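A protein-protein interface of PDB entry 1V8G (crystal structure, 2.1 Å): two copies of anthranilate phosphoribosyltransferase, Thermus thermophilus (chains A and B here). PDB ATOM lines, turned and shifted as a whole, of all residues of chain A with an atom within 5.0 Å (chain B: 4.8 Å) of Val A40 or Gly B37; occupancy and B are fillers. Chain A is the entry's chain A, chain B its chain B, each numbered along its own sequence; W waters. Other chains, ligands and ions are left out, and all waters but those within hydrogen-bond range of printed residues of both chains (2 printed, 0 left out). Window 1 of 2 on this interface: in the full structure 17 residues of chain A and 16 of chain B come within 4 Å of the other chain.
Hydrophobic or aromatic side chains of chain A within 4 Å of the printed part of chain B: Ala A36, Val A40, Ala A41, Leu A44 and Leu A167.
Of the 10 printed residues of chain B, 5 touch a printed residue of chain A.
Among the printed residues, 8 pairs touch across the chains.
Among the printed residues, no Asp or Glu carboxylate lies within 4 Å of a Lys or Arg side-chain nitrogen of the other chain.
OG of Ser A43 lies within hydrogen-bond range of O of Val A40 (3.0 Å).
Water W1 lies within hydrogen-bond range of the backbone carbonyl oxygen of Leu A167 (2.6 Å) and the guanidinium group of Arg B34 (3.0 Å).
Water W2 lies within hydrogen-bond range of the backbone carbonyl oxygen of Ile B8 (3.0 Å) and the side-chain hydroxyl of Ser A43 (3.3 Å).
Gly A37 touches Val B40, and with the chains exchanged Val A40 touches Gly B37.
Ala A41 touches Val B40, but with the chains exchanged Val A40 does not touch Ala B41 (4.1 Å).
7 positions are printed for both chains.
Of the 8 pairs that touch across the chains among the printed residues, 2 have their exchanged pair printed and touching as well.
Of chain B, only Ile B8 (3.8 Å) and Gly B37 (3.7 Å) come within 4 Å of Val A40.
Of the printed residues of chain B, Ala A36 touches Val B33 (3.5 Å).
Of the printed residues of chain B, Ala A41 touches Val B40.
The nearest printed residue of chain A that does not touch Ile B8 is Leu A167 (4.05 Å).
Among the printed residues, merely in contact across the chains: Ala A36 with Val B33, Gly A37 with Val B40, Val A40 with Ile B8, Val A40 with Gly B37, Ala A41 with Val B40, Leu A44 with Ile B8, Leu A44 with Ala B41 and Leu A167 with Val B33.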
ATOM      1  N   ALA A  35      25.616   5.756 -28.162  1.00  0.00           N
ATOM      2  CA  ALA A  35      24.331   5.796 -27.469  1.00  0.00           C
ATOM      3  C   ALA A  35      23.970   7.259 -27.240  1.00  0.00           C
ATOM      4  O   ALA A  35      22.850   7.676 -27.502  1.00  0.00           O
ATOM      5  CB  ALA A  35      24.418   5.056 -26.135  1.00  0.00           C
ATOM      6  N   ALA A  36      24.935   8.033 -26.757  1.00  0.00           N
ATOM      7  CA  ALA A  36      24.732   9.457 -26.519  1.00  0.00           C
ATOM      8  C   ALA A  36      24.316  10.137 -27.817  1.00  0.00           C
ATOM      9  O   ALA A  36      23.412  10.981 -27.836  1.00  0.00           O
ATOM     10  CB  ALA A  36      26.016  10.085 -25.997  1.00  0.00           C
ATOM     11  N   GLY A  37      24.979   9.769 -28.908  1.00  0.00           N
ATOM     12  CA  GLY A  37      24.650  10.356 -30.194  1.00  0.00           C
ATOM     13  C   GLY A  37      23.257  10.016 -30.702  1.00  0.00           C
ATOM     14  O   GLY A  37      22.536  10.895 -31.182  1.00  0.00           O
ATOM     15  N   LEU A  38      22.859   8.753 -30.607  1.00  0.00           N
ATOM     16  CA  LEU A  38      21.539   8.377 -31.106  1.00  0.00           C
ATOM     17  C   LEU A  38      20.436   8.988 -30.248  1.00  0.00           C
ATOM     18  O   LEU A  38      19.406   9.397 -30.768  1.00  0.00           O
ATOM     19  CB  LEU A  38      21.394   6.851 -31.184  1.00  0.00           C
ATOM     20  CG  LEU A  38      21.009   5.995 -29.981  1.00  0.00           C
ATOM     21  CD1 LEU A  38      19.499   6.056 -29.774  1.00  0.00           C
ATOM     22  CD2 LEU A  38      21.433   4.545 -30.241  1.00  0.00           C
ATOM     23  N   LEU A  39      20.662   9.069 -28.943  1.00  0.00           N
ATOM     24  CA  LEU A  39      19.671   9.659 -28.050  1.00  0.00           C
ATOM     25  C   LEU A  39      19.431  11.139 -28.374  1.00  0.00           C
ATOM     26  O   LEU A  39      18.286  11.605 -28.358  1.00  0.00           O
ATOM     27  CB  LEU A  39      20.114   9.497 -26.593  1.00  0.00           C
ATOM     28  CG  LEU A  39      20.102   8.045 -26.115  1.00  0.00           C
ATOM     29  CD1 LEU A  39      20.613   7.945 -24.678  1.00  0.00           C
ATOM     30  CD2 LEU A  39      18.681   7.500 -26.231  1.00  0.00           C
ATOM     31  N   VAL A  40      20.498  11.878 -28.673  1.00  0.00           N
ATOM     32  CA  VAL A  40      20.359  13.295 -29.014  1.00  0.00           C
ATOM     33  C   VAL A  40      19.661  13.444 -30.364  1.00  0.00           C
ATOM     34  O   VAL A  40      18.799  14.310 -30.534  1.00  0.00           O
ATOM     35  CB  VAL A  40      21.733  14.013 -29.062  1.00  0.00           C
ATOM     36  CG1 VAL A  40      21.583  15.422 -29.656  1.00  0.00           C
ATOM     37  CG2 VAL A  40      22.311  14.104 -27.658  1.00  0.00           C
ATOM     38  N   ALA A  41      20.029  12.595 -31.320  1.00  0.00           N
ATOM     39  CA  ALA A  41      19.431  12.636 -32.646  1.00  0.00           C
ATOM     40  C   ALA A  41      17.926  12.378 -32.565  1.00  0.00           C
ATOM     41  O   ALA A  41      17.146  13.050 -33.234  1.00  0.00           O
ATOM     42  CB  ALA A  41      20.089  11.599 -33.549  1.00  0.00           C
ATOM     43  N   LEU A  42      17.524  11.406 -31.745  1.00  0.00           N
ATOM     44  CA  LEU A  42      16.107  11.077 -31.592  1.00  0.00           C
ATOM     45  C   LEU A  42      15.314  12.200 -30.941  1.00  0.00           C
ATOM     46  O   LEU A  42      14.234  12.551 -31.411  1.00  0.00           O
ATOM     47  CB  LEU A  42      15.929   9.800 -30.769  1.00  0.00           C
ATOM     48  CG  LEU A  42      16.388   8.482 -31.403  1.00  0.00           C
ATOM     49  CD1 LEU A  42      15.870   7.309 -30.586  1.00  0.00           C
ATOM     50  CD2 LEU A  42      15.872   8.383 -32.812  1.00  0.00           C
ATOM     51  N   SER A  43      15.846  12.772 -29.865  1.00  0.00           N
ATOM     52  CA  SER A  43      15.141  13.849 -29.185  1.00  0.00           C
ATOM     53  C   SER A  43      15.034  15.097 -30.062  1.00  0.00           C
ATOM     54  O   SER A  43      14.051  15.830 -29.978  1.00  0.00           O
ATOM     55  CB  SER A  43      15.822  14.194 -27.854  1.00  0.00           C
ATOM     56  OG  SER A  43      17.176  14.557 -28.045  1.00  0.00           O
ATOM     57  N   LEU A  44      16.030  15.326 -30.916  1.00  0.00           N
ATOM     58  CA  LEU A  44      16.015  16.502 -31.781  1.00  0.00           C
ATOM     59  C   LEU A  44      15.020  16.434 -32.941  1.00  0.00           C
ATOM     60  O   LEU A  44      14.322  17.407 -33.209  1.00  0.00           O
ATOM     61  CB  LEU A  44      17.421  16.790 -32.319  1.00  0.00           C
ATOM     62  CG  LEU A  44      18.434  17.334 -31.302  1.00  0.00           C
ATOM     63  CD1 LEU A  44      19.751  17.638 -32.013  1.00  0.00           C
ATOM     64  CD2 LEU A  44      17.884  18.597 -30.639  1.00  0.00           C
ATOM     65  N   LEU A 167      24.452  13.487 -20.455  1.00  0.00           N
ATOM     66  CA  LEU A 167      23.910  14.346 -21.515  1.00  0.00           C
ATOM     67  C   LEU A 167      23.229  15.579 -20.936  1.00  0.00           C
ATOM     68  O   LEU A 167      23.250  16.655 -21.547  1.00  0.00           O
ATOM     69  CB  LEU A 167      22.897  13.585 -22.370  1.00  0.00           C
ATOM     70  CG  LEU A 167      23.442  12.659 -23.456  1.00  0.00           C
ATOM     71  CD1 LEU A 167      22.285  11.907 -24.076  1.00  0.00           C
ATOM     72  CD2 LEU A 167      24.189  13.474 -24.516  1.00  0.00           C
ATOM     73  N   ILE B   8      23.722  20.829 -27.479  1.00  0.00           N
ATOM     74  CA  ILE B   8      23.082  19.519 -27.387  1.00  0.00           C
ATOM     75  C   ILE B   8      21.567  19.660 -27.511  1.00  0.00           C
ATOM     76  O   ILE B   8      20.892  18.766 -28.028  1.00  0.00           O
ATOM     77  CB  ILE B   8      23.438  18.817 -26.053  1.00  0.00           C
ATOM     78  CG1 ILE B   8      24.935  18.489 -26.033  1.00  0.00           C
ATOM     79  CG2 ILE B   8      22.592  17.548 -25.871  1.00  0.00           C
ATOM     80  CD1 ILE B   8      25.439  17.902 -24.717  1.00  0.00           C
ATOM     81  N   VAL B  33      30.837  11.561 -24.120  1.00  0.00           N
ATOM     82  CA  VAL B  33      29.380  11.530 -24.263  1.00  0.00           C
ATOM     83  C   VAL B  33      28.839  12.866 -24.771  1.00  0.00           C
ATOM     84  O   VAL B  33      28.054  12.904 -25.721  1.00  0.00           O
ATOM     85  CB  VAL B  33      28.703  11.170 -22.916  1.00  0.00           C
ATOM     86  CG1 VAL B  33      27.212  11.505 -22.959  1.00  0.00           C
ATOM     87  CG2 VAL B  33      28.896   9.679 -22.631  1.00  0.00           C
ATOM     88  N   ARG B  34      29.265  13.961 -24.144  1.00  0.00           N
ATOM     89  CA  ARG B  34      28.807  15.286 -24.538  1.00  0.00           C
ATOM     90  C   ARG B  34      29.416  15.741 -25.855  1.00  0.00           C
ATOM     91  O   ARG B  34      28.789  16.482 -26.608  1.00  0.00           O
ATOM     92  CB  ARG B  34      29.097  16.294 -23.419  1.00  0.00           C
ATOM     93  CG  ARG B  34      28.430  15.904 -22.104  1.00  0.00           C
ATOM     94  CD  ARG B  34      28.700  16.912 -21.001  1.00  0.00           C
ATOM     95  NE  ARG B  34      27.868  18.099 -21.135  1.00  0.00           N
ATOM     96  CZ  ARG B  34      28.284  19.332 -20.875  1.00  0.00           C
ATOM     97  NH1 ARG B  34      29.533  19.543 -20.475  1.00  0.00           N
ATOM     98  NH2 ARG B  34      27.447  20.354 -21.001  1.00  0.00           N
ATOM     99  N   ALA B  35      30.636  15.300 -26.142  1.00  0.00           N
ATOM    100  CA  ALA B  35      31.263  15.661 -27.410  1.00  0.00           C
ATOM    101  C   ALA B  35      30.411  15.007 -28.492  1.00  0.00           C
ATOM    102  O   ALA B  35      30.110  15.608 -29.522  1.00  0.00           O
ATOM    103  CB  ALA B  35      32.697  15.121 -27.477  1.00  0.00           C
ATOM    104  N   ALA B  36      30.019  13.765 -28.238  1.00  0.00           N
ATOM    105  CA  ALA B  36      29.206  13.019 -29.182  1.00  0.00           C
ATOM    106  C   ALA B  36      27.852  13.690 -29.380  1.00  0.00           C
ATOM    107  O   ALA B  36      27.387  13.843 -30.510  1.00  0.00           O
ATOM    108  CB  ALA B  36      29.018  11.568 -28.683  1.00  0.00           C
ATOM    109  N   GLY B  37      27.213  14.081 -28.278  1.00  0.00           N
ATOM    110  CA  GLY B  37      25.905  14.709 -28.381  1.00  0.00           C
ATOM    111  C   GLY B  37      25.973  16.025 -29.125  1.00  0.00           C
ATOM    112  O   GLY B  37      25.151  16.320 -29.987  1.00  0.00           O
ATOM    113  N   LEU B  38      26.974  16.816 -28.766  1.00  0.00           N
ATOM    114  CA  LEU B  38      27.225  18.117 -29.363  1.00  0.00           C
ATOM    115  C   LEU B  38      27.402  18.038 -30.875  1.00  0.00           C
ATOM    116  O   LEU B  38      26.774  18.788 -31.622  1.00  0.00           O
ATOM    117  CB  LEU B  38      28.475  18.696 -28.705  1.00  0.00           C
ATOM    118  CG  LEU B  38      29.293  19.789 -29.366  1.00  0.00           C
ATOM    119  CD1 LEU B  38      28.486  21.075 -29.473  1.00  0.00           C
ATOM    120  CD2 LEU B  38      30.523  19.997 -28.510  1.00  0.00           C
ATOM    121  N   LEU B  39      28.254  17.120 -31.327  1.00  0.00           N
ATOM    122  CA  LEU B  39      28.518  16.951 -32.754  1.00  0.00           C
ATOM    123  C   LEU B  39      27.286  16.477 -33.537  1.00  0.00           C
ATOM    124  O   LEU B  39      27.057  16.910 -34.665  1.00  0.00           O
ATOM    125  CB  LEU B  39      29.687  15.980 -32.959  1.00  0.00           C
ATOM    126  CG  LEU B  39      31.053  16.483 -32.479  1.00  0.00           C
ATOM    127  CD1 LEU B  39      32.117  15.393 -32.624  1.00  0.00           C
ATOM    128  CD2 LEU B  39      31.442  17.709 -33.288  1.00  0.00           C
ATOM    129  N   VAL B  40      26.493  15.588 -32.945  1.00  0.00           N
ATOM    130  CA  VAL B  40      25.292  15.111 -33.624  1.00  0.00           C
ATOM    131  C   VAL B  40      24.300  16.255 -33.784  1.00  0.00           C
ATOM    132  O   VAL B  40      23.762  16.473 -34.873  1.00  0.00           O
ATOM    133  CB  VAL B  40      24.625  13.963 -32.842  1.00  0.00           C
ATOM    134  CG1 VAL B  40      23.209  13.718 -33.371  1.00  0.00           C
ATOM    135  CG2 VAL B  40      25.462  12.708 -32.989  1.00  0.00           C
ATOM    136  N   ALA B  41      24.072  16.991 -32.697  1.00  0.00           N
ATOM    137  CA  ALA B  41      23.151  18.117 -32.722  1.00  0.00           C
ATOM    138  C   ALA B  41      23.506  19.127 -33.815  1.00  0.00           C
ATOM    139  O   ALA B  41      22.624  19.630 -34.515  1.00  0.00           O
ATOM    140  CB  ALA B  41      23.136  18.811 -31.356  1.00  0.00           C
HETATM  141  O   HOH W   1      24.882  18.658 -21.158  1.00  0.00           O
HETATM  142  O   HOH W   2      18.447  17.422 -26.944  1.00  0.00           O
